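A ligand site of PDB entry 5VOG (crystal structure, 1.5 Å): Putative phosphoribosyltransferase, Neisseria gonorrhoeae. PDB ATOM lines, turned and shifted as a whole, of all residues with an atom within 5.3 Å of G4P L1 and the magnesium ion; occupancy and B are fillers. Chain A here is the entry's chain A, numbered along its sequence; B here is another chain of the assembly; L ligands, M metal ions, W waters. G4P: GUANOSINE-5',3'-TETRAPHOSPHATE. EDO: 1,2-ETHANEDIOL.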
ATOM      1  N   ILE A  44       9.826 -20.000 -23.848  1.00  0.00           N
ATOM      2  CA  ILE A  44       9.990 -19.323 -22.563  1.00  0.00           C
ATOM      3  C   ILE A  44       8.872 -19.807 -21.644  1.00  0.00           C
ATOM      4  O   ILE A  44       7.713 -19.410 -21.800  1.00  0.00           O
ATOM      5  CB  ILE A  44       9.948 -17.793 -22.712  1.00  0.00           C
ATOM      6  CG1 ILE A  44      10.982 -17.316 -23.744  1.00  0.00           C
ATOM      7  CG2 ILE A  44      10.190 -17.133 -21.360  1.00  0.00           C
ATOM      8  CD1 ILE A  44      10.808 -15.844 -24.134  1.00  0.00           C
ATOM      9  N   GLY A  45       9.204 -20.658 -20.666  1.00  0.00           N
ATOM     10  CA  GLY A  45       8.193 -21.106 -19.726  1.00  0.00           C
ATOM     11  C   GLY A  45       7.874 -20.037 -18.695  1.00  0.00           C
ATOM     12  O   GLY A  45       8.669 -19.126 -18.472  1.00  0.00           O
ATOM     13  N   GLY A  46       6.705 -20.133 -18.060  1.00  0.00           N
ATOM     14  CA  GLY A  46       5.752 -21.207 -18.275  1.00  0.00           C
ATOM     15  C   GLY A  46       4.766 -20.949 -19.409  1.00  0.00           C
ATOM     16  O   GLY A  46       4.162 -21.891 -19.925  1.00  0.00           O
ATOM     17  N   GLY A  47       4.634 -19.672 -19.798  1.00  0.00           N
ATOM     18  CA  GLY A  47       3.596 -19.303 -20.749  1.00  0.00           C
ATOM     19  C   GLY A  47       3.857 -19.786 -22.160  1.00  0.00           C
ATOM     20  O   GLY A  47       2.908 -19.999 -22.934  1.00  0.00           O
ATOM     21  N   GLY A  48       5.120 -19.991 -22.535  1.00  0.00           N
ATOM     22  CA  GLY A  48       5.434 -20.402 -23.888  1.00  0.00           C
ATOM     23  C   GLY A  48       5.363 -21.900 -24.151  1.00  0.00           C
ATOM     24  O   GLY A  48       5.451 -22.316 -25.307  1.00  0.00           O
ATOM     25  N   THR A  68      11.721 -17.690 -17.238  1.00  0.00           N
ATOM     26  CA  THR A  68      11.948 -16.454 -16.519  1.00  0.00           C
ATOM     27  C   THR A  68      10.800 -16.239 -15.542  1.00  0.00           C
ATOM     28  O   THR A  68       9.703 -16.790 -15.706  1.00  0.00           O
ATOM     29  CB  THR A  68      12.026 -15.261 -17.472  1.00  0.00           C
ATOM     30  OG1 THR A  68      10.829 -15.212 -18.259  1.00  0.00           O
ATOM     31  CG2 THR A  68      13.224 -15.387 -18.377  1.00  0.00           C
ATOM     32  N   ALA A  69      11.040 -15.393 -14.550  1.00  0.00           N
ATOM     33  CA  ALA A  69       9.989 -14.978 -13.630  1.00  0.00           C
ATOM     34  C   ALA A  69      10.323 -13.586 -13.118  1.00  0.00           C
ATOM     35  O   ALA A  69      11.474 -13.147 -13.182  1.00  0.00           O
ATOM     36  CB  ALA A  69       9.828 -15.967 -12.472  1.00  0.00           C
ATOM     37  N   TYR A  70       9.309 -12.888 -12.647  1.00  0.00           N
ATOM     38  CA  TYR A  70       9.529 -11.613 -11.986  1.00  0.00           C
ATOM     39  C   TYR A  70       9.795 -11.840 -10.510  1.00  0.00           C
ATOM     40  O   TYR A  70       9.184 -12.717  -9.879  1.00  0.00           O
ATOM     41  CB  TYR A  70       8.330 -10.678 -12.175  1.00  0.00           C
ATOM     42  CG  TYR A  70       8.250 -10.023 -13.537  1.00  0.00           C
ATOM     43  CD1 TYR A  70       8.651  -8.703 -13.718  1.00  0.00           C
ATOM     44  CD2 TYR A  70       7.760 -10.714 -14.638  1.00  0.00           C
ATOM     45  CE1 TYR A  70       8.561  -8.094 -14.952  1.00  0.00           C
ATOM     46  CE2 TYR A  70       7.667 -10.106 -15.896  1.00  0.00           C
ATOM     47  CZ  TYR A  70       8.069  -8.789 -16.039  1.00  0.00           C
ATOM     48  OH  TYR A  70       7.987  -8.175 -17.263  1.00  0.00           O
ATOM     49  N   ASP A 105       6.681 -17.455 -27.113  1.00  0.00           N
ATOM     50  CA  ASP A 105       6.014 -17.103 -25.863  1.00  0.00           C
ATOM     51  C   ASP A 105       4.525 -16.913 -26.141  1.00  0.00           C
ATOM     52  O   ASP A 105       4.095 -16.882 -27.300  1.00  0.00           O
ATOM     53  CB  ASP A 105       6.622 -15.848 -25.223  1.00  0.00           C
ATOM     54  CG  ASP A 105       6.654 -15.922 -23.708  1.00  0.00           C
ATOM     55  OD1 ASP A 105       5.809 -16.637 -23.127  1.00  0.00           O
ATOM     56  OD2 ASP A 105       7.504 -15.239 -23.088  1.00  0.00           O
ATOM     57  N   GLU A 106       3.720 -16.823 -25.070  1.00  0.00           N
ATOM     58  CA  GLU A 106       2.268 -16.761 -25.304  1.00  0.00           C
ATOM     59  C   GLU A 106       1.755 -15.344 -25.526  1.00  0.00           C
ATOM     60  O   GLU A 106       0.860 -15.148 -26.353  1.00  0.00           O
ATOM     61  CB  GLU A 106       1.480 -17.457 -24.177  1.00  0.00           C
ATOM     62  CG  GLU A 106       0.929 -16.597 -23.041  1.00  0.00           C
ATOM     63  CD  GLU A 106       1.967 -16.219 -22.002  1.00  0.00           C
ATOM     64  OE1 GLU A 106       3.124 -15.955 -22.380  1.00  0.00           O
ATOM     65  OE2 GLU A 106       1.637 -16.176 -20.795  1.00  0.00           O
ATOM     66  N   VAL A 107       2.278 -14.332 -24.824  1.00  0.00           N
ATOM     67  CA  VAL A 107       1.714 -12.990 -24.914  1.00  0.00           C
ATOM     68  C   VAL A 107       2.810 -11.952 -24.967  1.00  0.00           C
ATOM     69  O   VAL A 107       3.807 -12.039 -24.239  1.00  0.00           O
ATOM     70  CB  VAL A 107       0.704 -12.687 -23.770  1.00  0.00           C
ATOM     71  CG1 VAL A 107       1.373 -12.594 -22.400  1.00  0.00           C
ATOM     72  CG2 VAL A 107      -0.070 -11.405 -24.074  1.00  0.00           C
ATOM     73  N   ASP A 108       2.652 -10.992 -25.883  1.00  0.00           N
ATOM     74  CA  ASP A 108       3.443  -9.778 -25.990  1.00  0.00           C
ATOM     75  C   ASP A 108       2.625  -8.684 -25.314  1.00  0.00           C
ATOM     76  O   ASP A 108       1.682  -8.134 -25.902  1.00  0.00           O
ATOM     77  CB  ASP A 108       3.722  -9.496 -27.470  1.00  0.00           C
ATOM     78  CG  ASP A 108       4.479  -8.197 -27.702  1.00  0.00           C
ATOM     79  OD1 ASP A 108       4.526  -7.331 -26.810  1.00  0.00           O
ATOM     80  OD2 ASP A 108       4.996  -8.055 -28.828  1.00  0.00           O
ATOM     81  N   ASP A 109       2.962  -8.399 -24.060  1.00  0.00           N
ATOM     82  CA  ASP A 109       2.250  -7.412 -23.249  1.00  0.00           C
ATOM     83  C   ASP A 109       3.125  -6.189 -23.043  1.00  0.00           C
ATOM     84  O   ASP A 109       2.876  -5.144 -23.657  1.00  0.00           O
ATOM     85  CB  ASP A 109       1.829  -8.032 -21.919  1.00  0.00           C
ATOM     86  CG  ASP A 109       0.968  -7.109 -21.080  1.00  0.00           C
ATOM     87  OD1 ASP A 109      -0.093  -6.688 -21.585  1.00  0.00           O
ATOM     88  OD2 ASP A 109       1.330  -6.831 -19.922  1.00  0.00           O
ATOM     89  N   SER A 110       4.167  -6.279 -22.207  1.00  0.00           N
ATOM     90  CA  SER A 110       5.065  -5.153 -21.989  1.00  0.00           C
ATOM     91  C   SER A 110       6.373  -5.252 -22.761  1.00  0.00           C
ATOM     92  O   SER A 110       7.084  -4.252 -22.879  1.00  0.00           O
ATOM     93  CB  SER A 110       5.421  -5.035 -20.487  1.00  0.00           C
ATOM     94  OG  SER A 110       6.338  -6.062 -20.105  1.00  0.00           O
ATOM     95  N   ARG A 111       6.711  -6.439 -23.276  1.00  0.00           N
ATOM     96  CA  ARG A 111       7.970  -6.770 -23.936  1.00  0.00           C
ATOM     97  C   ARG A 111       9.179  -6.756 -23.004  1.00  0.00           C
ATOM     98  O   ARG A 111      10.308  -6.899 -23.474  1.00  0.00           O
ATOM     99  CB  ARG A 111       8.271  -5.870 -25.136  1.00  0.00           C
ATOM    100  CG  ARG A 111       7.480  -6.258 -26.333  1.00  0.00           C
ATOM    101  CD  ARG A 111       7.681  -5.339 -27.512  1.00  0.00           C
ATOM    102  NE  ARG A 111       6.732  -5.757 -28.528  1.00  0.00           N
ATOM    103  CZ  ARG A 111       6.441  -5.077 -29.635  1.00  0.00           C
ATOM    104  NH1 ARG A 111       7.043  -3.911 -29.885  1.00  0.00           N
ATOM    105  NH2 ARG A 111       5.554  -5.567 -30.476  1.00  0.00           N
ATOM    106  N   VAL A 112       8.972  -6.623 -21.693  1.00  0.00           N
ATOM    107  CA  VAL A 112      10.102  -6.631 -20.771  1.00  0.00           C
ATOM    108  C   VAL A 112      10.764  -8.020 -20.733  1.00  0.00           C
ATOM    109  O   VAL A 112      11.992  -8.123 -20.787  1.00  0.00           O
ATOM    110  CB  VAL A 112       9.669  -6.143 -19.376  1.00  0.00           C
ATOM    111  CG1 VAL A 112      10.773  -6.354 -18.352  1.00  0.00           C
ATOM    112  CG2 VAL A 112       9.312  -4.652 -19.453  1.00  0.00           C
ATOM    113  N   THR A 113       9.970  -9.093 -20.682  1.00  0.00           N
ATOM    114  CA  THR A 113      10.572 -10.419 -20.706  1.00  0.00           C
ATOM    115  C   THR A 113      11.202 -10.691 -22.069  1.00  0.00           C
ATOM    116  O   THR A 113      12.307 -11.253 -22.154  1.00  0.00           O
ATOM    117  CB  THR A 113       9.538 -11.499 -20.402  1.00  0.00           C
ATOM    118  OG1 THR A 113       9.045 -11.312 -19.072  1.00  0.00           O
ATOM    119  CG2 THR A 113      10.167 -12.908 -20.515  1.00  0.00           C
ATOM    120  N   MET A 114      10.481 -10.325 -23.127  1.00  0.00           N
ATOM    121  CA  MET A 114      10.963 -10.581 -24.481  1.00  0.00           C
ATOM    122  C   MET A 114      12.312  -9.910 -24.721  1.00  0.00           C
ATOM    123  O   MET A 114      13.243 -10.529 -25.248  1.00  0.00           O
ATOM    124  CB  MET A 114       9.925 -10.106 -25.490  1.00  0.00           C
ATOM    125  CG  MET A 114      10.206 -10.530 -26.915  1.00  0.00           C
ATOM    126  SD  MET A 114       8.985  -9.802 -28.030  1.00  0.00           S
ATOM    127  CE  MET A 114       7.510 -10.602 -27.428  1.00  0.00           C
ATOM    128  N   GLU A 115      12.430  -8.630 -24.350  1.00  0.00           N
ATOM    129  CA  GLU A 115      13.708  -7.929 -24.521  1.00  0.00           C
ATOM    130  C   GLU A 115      14.812  -8.600 -23.728  1.00  0.00           C
ATOM    131  O   GLU A 115      15.928  -8.775 -24.219  1.00  0.00           O
ATOM    132  CB  GLU A 115      13.588  -6.462 -24.107  1.00  0.00           C
ATOM    133  CG  GLU A 115      14.935  -5.733 -24.191  1.00  0.00           C
ATOM    134  CD  GLU A 115      14.930  -4.323 -23.609  1.00  0.00           C
ATOM    135  OE1 GLU A 115      13.929  -3.601 -23.721  1.00  0.00           O
ATOM    136  OE2 GLU A 115      15.976  -3.924 -23.049  1.00  0.00           O
ATOM    137  N   LYS A 137      -0.536  -7.844 -27.882  1.00  0.00           N
ATOM    138  CA  LYS A 137      -1.404  -6.762 -27.413  1.00  0.00           C
ATOM    139  C   LYS A 137      -0.948  -5.420 -27.977  1.00  0.00           C
ATOM    140  O   LYS A 137       0.243  -5.097 -27.932  1.00  0.00           O
ATOM    141  CB  LYS A 137      -1.422  -6.696 -25.896  1.00  0.00           C
ATOM    142  CG  LYS A 137      -2.082  -7.861 -25.217  1.00  0.00           C
ATOM    143  CD  LYS A 137      -2.082  -7.557 -23.740  1.00  0.00           C
ATOM    144  CE  LYS A 137      -2.782  -8.572 -22.931  1.00  0.00           C
ATOM    145  NZ  LYS A 137      -2.785  -8.118 -21.513  1.00  0.00           N
ATOM    146  N   TRP A 160      -6.619  -5.879 -23.753  1.00  0.00           N
ATOM    147  CA  TRP A 160      -7.584  -6.559 -22.908  1.00  0.00           C
ATOM    148  C   TRP A 160      -6.868  -7.619 -22.096  1.00  0.00           C
ATOM    149  O   TRP A 160      -5.795  -8.106 -22.477  1.00  0.00           O
ATOM    150  CB  TRP A 160      -8.680  -7.242 -23.739  1.00  0.00           C
ATOM    151  CG  TRP A 160      -9.561  -6.315 -24.525  1.00  0.00           C
ATOM    152  CD1 TRP A 160      -9.548  -4.953 -24.533  1.00  0.00           C
ATOM    153  CD2 TRP A 160     -10.603  -6.710 -25.426  1.00  0.00           C
ATOM    154  NE1 TRP A 160     -10.511  -4.484 -25.388  1.00  0.00           N
ATOM    155  CE2 TRP A 160     -11.170  -5.538 -25.953  1.00  0.00           C
ATOM    156  CE3 TRP A 160     -11.104  -7.959 -25.841  1.00  0.00           C
ATOM    157  CZ2 TRP A 160     -12.220  -5.562 -26.858  1.00  0.00           C
ATOM    158  CZ3 TRP A 160     -12.143  -7.974 -26.748  1.00  0.00           C
ATOM    159  CH2 TRP A 160     -12.686  -6.790 -27.250  1.00  0.00           C
ATOM    160  N   TRP A 161      -7.472  -8.020 -20.982  1.00  0.00           N
ATOM    161  CA  TRP A 161      -6.915  -9.128 -20.224  1.00  0.00           C
ATOM    162  C   TRP A 161      -7.344 -10.443 -20.864  1.00  0.00           C
ATOM    163  O   TRP A 161      -8.555 -10.702 -21.007  1.00  0.00           O
ATOM    164  CB  TRP A 161      -7.351  -9.091 -18.762  1.00  0.00           C
ATOM    165  CG  TRP A 161      -6.577 -10.104 -17.983  1.00  0.00           C
ATOM    166  CD1 TRP A 161      -7.014 -11.310 -17.523  1.00  0.00           C
ATOM    167  CD2 TRP A 161      -5.201  -9.995 -17.605  1.00  0.00           C
ATOM    168  NE1 TRP A 161      -5.990 -11.966 -16.866  1.00  0.00           N
ATOM    169  CE2 TRP A 161      -4.871 -11.187 -16.913  1.00  0.00           C
ATOM    170  CE3 TRP A 161      -4.213  -9.030 -17.790  1.00  0.00           C
ATOM    171  CZ2 TRP A 161      -3.599 -11.410 -16.385  1.00  0.00           C
ATOM    172  CZ3 TRP A 161      -2.938  -9.258 -17.271  1.00  0.00           C
ATOM    173  CH2 TRP A 161      -2.649 -10.438 -16.584  1.00  0.00           C
ATOM    174  N   ILE A 162      -6.380 -11.257 -21.240  1.00  0.00           N
ATOM    175  CA  ILE A 162      -6.634 -12.533 -21.886  1.00  0.00           C
ATOM    176  C   ILE A 162      -6.679 -13.623 -20.839  1.00  0.00           C
ATOM    177  O   ILE A 162      -5.736 -13.773 -20.046  1.00  0.00           O
ATOM    178  CB  ILE A 162      -5.563 -12.830 -22.946  1.00  0.00           C
ATOM    179  CG1 ILE A 162      -5.542 -11.741 -24.022  1.00  0.00           C
ATOM    180  CG2 ILE A 162      -5.782 -14.210 -23.549  1.00  0.00           C
ATOM    181  CD1 ILE A 162      -4.299 -11.798 -24.917  1.00  0.00           C
ATOM    182  N   ASN A 163      -7.768 -14.388 -20.827  1.00  0.00           N
ATOM    183  CA  ASN A 163      -7.907 -15.537 -19.927  1.00  0.00           C
ATOM    184  C   ASN A 163      -7.619 -16.806 -20.717  1.00  0.00           C
ATOM    185  O   ASN A 163      -8.369 -17.144 -21.636  1.00  0.00           O
ATOM    186  CB  ASN A 163      -9.294 -15.553 -19.303  1.00  0.00           C
ATOM    187  CG  ASN A 163      -9.544 -14.343 -18.447  1.00  0.00           C
ATOM    188  OD1 ASN A 163      -9.117 -14.299 -17.295  1.00  0.00           O
ATOM    189  ND2 ASN A 163     -10.199 -13.327 -19.007  1.00  0.00           N
ATOM    190  N   TYR A 164      -6.516 -17.489 -20.362  1.00  0.00           N
ATOM    191  CA  TYR A 164      -6.062 -18.685 -21.050  1.00  0.00           C
ATOM    192  C   TYR A 164      -6.740 -19.930 -20.486  1.00  0.00           C
ATOM    193  O   TYR A 164      -6.981 -20.008 -19.281  1.00  0.00           O
ATOM    194  CB  TYR A 164      -4.542 -18.829 -20.941  1.00  0.00           C
ATOM    195  CG  TYR A 164      -3.848 -17.779 -21.771  1.00  0.00           C
ATOM    196  CD1 TYR A 164      -3.811 -17.899 -23.149  1.00  0.00           C
ATOM    197  CD2 TYR A 164      -3.301 -16.641 -21.190  1.00  0.00           C
ATOM    198  CE1 TYR A 164      -3.207 -16.933 -23.935  1.00  0.00           C
ATOM    199  CE2 TYR A 164      -2.701 -15.656 -21.964  1.00  0.00           C
ATOM    200  CZ  TYR A 164      -2.673 -15.808 -23.339  1.00  0.00           C
ATOM    201  OH  TYR A 164      -2.087 -14.833 -24.135  1.00  0.00           O
ATOM    202  N   ASP A 167      -5.308 -21.770 -17.454  1.00  0.00           N
ATOM    203  CA  ASP A 167      -5.520 -21.211 -16.129  1.00  0.00           C
ATOM    204  C   ASP A 167      -6.934 -21.456 -15.600  1.00  0.00           C
ATOM    205  O   ASP A 167      -7.300 -20.917 -14.554  1.00  0.00           O
ATOM    206  CB  ASP A 167      -5.247 -19.708 -16.128  1.00  0.00           C
ATOM    207  CG  ASP A 167      -3.777 -19.378 -16.289  1.00  0.00           C
ATOM    208  OD1 ASP A 167      -2.931 -20.084 -15.691  1.00  0.00           O
ATOM    209  OD2 ASP A 167      -3.475 -18.406 -17.024  1.00  0.00           O
ATOM    210  N   ARG B  53       2.095 -27.713 -17.882  1.00  0.00           N
ATOM    211  CA  ARG B  53       1.511 -26.378 -17.728  1.00  0.00           C
ATOM    212  C   ARG B  53       0.038 -26.467 -17.322  1.00  0.00           C
ATOM    213  O   ARG B  53      -0.432 -25.628 -16.539  1.00  0.00           O
ATOM    214  CB  ARG B  53       1.690 -25.552 -19.003  1.00  0.00           C
ATOM    215  CG  ARG B  53       1.102 -24.138 -18.893  1.00  0.00           C
ATOM    216  CD  ARG B  53       1.718 -23.351 -17.739  1.00  0.00           C
ATOM    217  NE  ARG B  53       1.131 -22.023 -17.535  1.00  0.00           N
ATOM    218  CZ  ARG B  53      -0.005 -21.790 -16.892  1.00  0.00           C
ATOM    219  NH1 ARG B  53      -0.715 -22.796 -16.372  1.00  0.00           N
ATOM    220  NH2 ARG B  53      -0.446 -20.543 -16.755  1.00  0.00           N
ATOM    221  N   ARG B  56       0.120 -26.970 -13.687  1.00  0.00           N
ATOM    222  CA  ARG B  56       0.469 -25.780 -12.908  1.00  0.00           C
ATOM    223  C   ARG B  56      -0.771 -24.995 -12.501  1.00  0.00           C
ATOM    224  O   ARG B  56      -0.759 -24.314 -11.471  1.00  0.00           O
ATOM    225  CB  ARG B  56       1.427 -24.874 -13.691  1.00  0.00           C
ATOM    226  CG  ARG B  56       2.269 -23.990 -12.794  1.00  0.00           C
ATOM    227  CD  ARG B  56       3.147 -23.043 -13.598  1.00  0.00           C
ATOM    228  NE  ARG B  56       2.424 -21.832 -13.967  1.00  0.00           N
ATOM    229  CZ  ARG B  56       2.967 -20.797 -14.608  1.00  0.00           C
ATOM    230  NH1 ARG B  56       4.225 -20.829 -14.997  1.00  0.00           N
ATOM    231  NH2 ARG B  56       2.217 -19.737 -14.880  1.00  0.00           N
HETATM  232  PB  G4P L   1       6.386  -9.985 -22.736  1.00  0.00           P
HETATM  233  O1B G4P L   1       7.771  -9.593 -22.615  1.00  0.00           O
HETATM  234  O2B G4P L   1       5.442  -8.906 -23.306  1.00  0.00           O
HETATM  235  O3B G4P L   1       6.244 -11.301 -23.574  1.00  0.00           O
HETATM  236  O3A G4P L   1       5.791 -10.435 -21.324  1.00  0.00           O
HETATM  237  PA  G4P L   1       5.698  -9.664 -19.940  1.00  0.00           P
HETATM  238  O1A G4P L   1       7.026  -9.559 -19.293  1.00  0.00           O
HETATM  239  O2A G4P L   1       4.991  -8.349 -20.149  1.00  0.00           O
HETATM  240  O5' G4P L   1       4.680 -10.631 -19.153  1.00  0.00           O
HETATM  241  C5' G4P L   1       4.648 -10.715 -17.710  1.00  0.00           C
HETATM  242  C4' G4P L   1       3.566 -11.692 -17.322  1.00  0.00           C
HETATM  243  O4' G4P L   1       2.271 -11.126 -17.585  1.00  0.00           O
HETATM  244  C3' G4P L   1       3.613 -13.029 -18.084  1.00  0.00           C
HETATM  245  O3' G4P L   1       3.743 -14.097 -17.118  1.00  0.00           O
HETATM  246  C2' G4P L   1       2.278 -13.115 -18.826  1.00  0.00           C
HETATM  247  O2' G4P L   1       1.726 -14.435 -18.865  1.00  0.00           O
HETATM  248  C1' G4P L   1       1.410 -12.158 -18.008  1.00  0.00           C
HETATM  249  N9  G4P L   1       0.353 -11.553 -18.811  1.00  0.00           N
HETATM  250  C8  G4P L   1       0.429 -10.393 -19.547  1.00  0.00           C
HETATM  251  N7  G4P L   1      -0.686 -10.112 -20.179  1.00  0.00           N
HETATM  252  C5  G4P L   1      -1.543 -11.148 -19.848  1.00  0.00           C
HETATM  253  C6  G4P L   1      -2.903 -11.399 -20.214  1.00  0.00           C
HETATM  254  O6  G4P L   1      -3.622 -10.714 -20.941  1.00  0.00           O
HETATM  255  N1  G4P L   1      -3.391 -12.555 -19.644  1.00  0.00           N
HETATM  256  C2  G4P L   1      -2.681 -13.390 -18.815  1.00  0.00           C
HETATM  257  N2  G4P L   1      -3.316 -14.456 -18.334  1.00  0.00           N
HETATM  258  N3  G4P L   1      -1.416 -13.166 -18.472  1.00  0.00           N
HETATM  259  C4  G4P L   1      -0.914 -12.040 -19.011  1.00  0.00           C
HETATM  260  PC  G4P L   1       5.135 -14.546 -16.527  1.00  0.00           P
HETATM  261  O1C G4P L   1       5.546 -13.657 -15.404  1.00  0.00           O
HETATM  262  O2C G4P L   1       6.076 -14.565 -17.704  1.00  0.00           O
HETATM  263  O3C G4P L   1       4.902 -16.046 -16.038  1.00  0.00           O
HETATM  264  PD  G4P L   1       4.584 -17.421 -16.777  1.00  0.00           P
HETATM  265  O1D G4P L   1       4.919 -17.203 -18.219  1.00  0.00           O
HETATM  266  O2D G4P L   1       5.490 -18.467 -16.106  1.00  0.00           O
HETATM  267  O3D G4P L   1       3.132 -17.702 -16.497  1.00  0.00           O
HETATM  268  C1  EDO L   2       6.532 -13.434 -20.697  1.00  0.00           C
HETATM  269  O1  EDO L   2       7.274 -14.638 -20.443  1.00  0.00           O
HETATM  270  C2  EDO L   2       5.163 -13.824 -21.247  1.00  0.00           C
HETATM  271  O2  EDO L   2       4.752 -14.999 -20.527  1.00  0.00           O
HETATM  272 MG    MG M   1       6.173 -15.978 -19.255  1.00  0.00          MG
HETATM  273  O   HOH W   1      -5.352 -16.635 -17.929  1.00  0.00           O
HETATM  274  O   HOH W   2       8.863 -13.547 -17.291  1.00  0.00           O
HETATM  275  O   HOH W   3       7.480 -17.856 -14.469  1.00  0.00           O
HETATM  276  O   HOH W   4       1.005  -8.616 -16.210  1.00  0.00           O
HETATM  277  O   HOH W   5       8.659 -12.961 -24.113  1.00  0.00           O
HETATM  278  O   HOH W   6      -1.508 -16.797 -17.691  1.00  0.00           O
HETATM  279  O   HOH W   7       3.454 -12.656 -13.843  1.00  0.00           O
HETATM  280  O   HOH W   8      -0.786 -14.091 -15.847  1.00  0.00           O
HETATM  281  O   HOH W   9       1.011 -16.035 -16.747  1.00  0.00           O
HETATM  282  O   HOH W  10       6.292 -17.327 -20.705  1.00  0.00           O
HETATM  283  O   HOH W  11       2.886 -16.522 -13.502  1.00  0.00           O
HETATM  284  O   HOH W  12       7.911 -16.656 -18.314  1.00  0.00           O
HETATM  285  O   HOH W  13       3.120  -7.455 -18.303  1.00  0.00           O
HETATM  286  O   HOH W  14       6.674 -13.962 -13.033  1.00  0.00           O
HETATM  287  O   HOH W  15       1.674 -19.219 -18.209  1.00  0.00           O
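An oxygen (O2') of G4P L1 is in hydrogen-bond range of the side-chain carboxylate of Glu 106, 2.6 Å away. The backbone carbonyl oxygen of Val 107 sits close to an oxygen (O3B) of G4P L1 (2.6 Å). The side-chain hydroxyl (OH) of Tyr 70 sits at hydrogen-bond distance from an oxygen (O1A) of G4P L1. The backbone NH (N) of Asp 109 lies within hydrogen-bond range of an oxygen (O2B) of G4P L1. O2A of G4P L1 sits at hydrogen-bond distance from N of Ser 110. OG of Ser 110 sits at hydrogen-bond distance from O2A of G4P L1. N of Ile 162 lies within hydrogen-bond range of O6 of G4P L1 (2.8 Å). The backbone carbonyl oxygen of Ile 162 lies within hydrogen-bond range of a nitrogen (N1) of G4P L1. The backbone NH of Thr 113 lies within hydrogen-bond range of an oxygen (O1B) of G4P L1. The side-chain hydroxyl (OG1) of Thr 113 is in hydrogen-bond range of an oxygen (O1A) of G4P L1. NH2 of Arg 56 of chain B lies within salt-bridge range of O3D of G4P L1, at 2.8 Å. The backbone NH (N) of Arg 111 is in hydrogen-bond range of an oxygen (O2B) of G4P L1 (2.8 Å). The side-chain amino group (NZ) of Lys 137 sits at hydrogen-bond distance from an oxygen (O6) of G4P L1 (2.8 Å). N of Gly 46 sits at hydrogen-bond distance from O2D of G4P L1, at 2.8 Å. The backbone NH of Met 114 is in hydrogen-bond range of an oxygen (O1B) of G4P L1. The backbone NH (N) of Gly 47 lies close to an oxygen (O1D) of G4P L1 (2.9 Å). N of Val 112 sits at hydrogen-bond distance from O1B of G4P L1 (3.3 Å).
Residues that only touch G4P L1: Gly 45 (3.9 Å), Asp 108 (3.5 Å), Trp 160 (3.7 Å), Trp 161 (3.3 Å) and Tyr 164 (3.6 Å). Hydrophobic or aromatic side chains that line G4P L1: Tyr 70, Val 107, Met 114, Trp 161, Ile 162 and Tyr 164. The nearest printed residue that does not touch G4P L1 is Asp 105 (4.2 Å).
OD1 of Asp 105 touches the magnesium ion, 3.9 Å away.
Water W12 bridges the backbone carbonyl oxygen (O) of Gly 45 (2.6 Å) and the backbone carbonyl oxygen (O) of Thr 68 (3.2 Å). Water W14 lies within hydrogen-bond range of an oxygen (O1C) of G4P L1 (2.6 Å) and the backbone NH of Tyr 70 (2.9 Å). Water W3 bridges O2D of G4P L1 (2.6 Å) and O of Thr 68 (2.8 Å). Water W5 lies within hydrogen-bond range of OD2 of Asp 105 (2.8 Å), O3B of G4P L1 (3.0 Å) and N of Met 114 (3.4 Å). Water W2 lies within hydrogen-bond range of OG1 of Thr 68 (2.8 Å) and OG1 of Thr 113 (2.9 Å). Water W6 lies within hydrogen-bond range of OD2 of Asp 167 (2.6 Å) and N2 of G4P L1 (3.0 Å).
OD1 of Asp 109 is in salt-bridge range of NZ of Lys 137, at 3.0 Å. The side-chain hydroxyl of Ser 110 is in hydrogen-bond range of the backbone NH of Val 112. The side-chain carboxylate of Asp 108 lies within salt-bridge range of the guanidinium group of Arg 111, 2.9 Å away. O of Asp 108 sits at hydrogen-bond distance from N of Lys 137, 3.0 Å away. The side-chain amino group (NZ) of Lys 137 sits close to the backbone carbonyl oxygen (O) of Trp 160 (3.2 Å). The side-chain carboxylate (OD1) of Asp 105 sits at hydrogen-bond distance from the backbone NH (N) of Gly 48, at 3.5 Å.
The magnesium ion is bound by water W10 (2.0 Å), an oxygen (O1D) of G4P L1 (2.0 Å), water W12 (2.1 Å), an oxygen (O2C) of G4P L1 (2.1 Å), an oxygen (O1) of EDO L2 (2.1 Å) and an oxygen (O2) of EDO L2 (2.1 Å). The magnesium ion has six donor atoms within binding distance.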
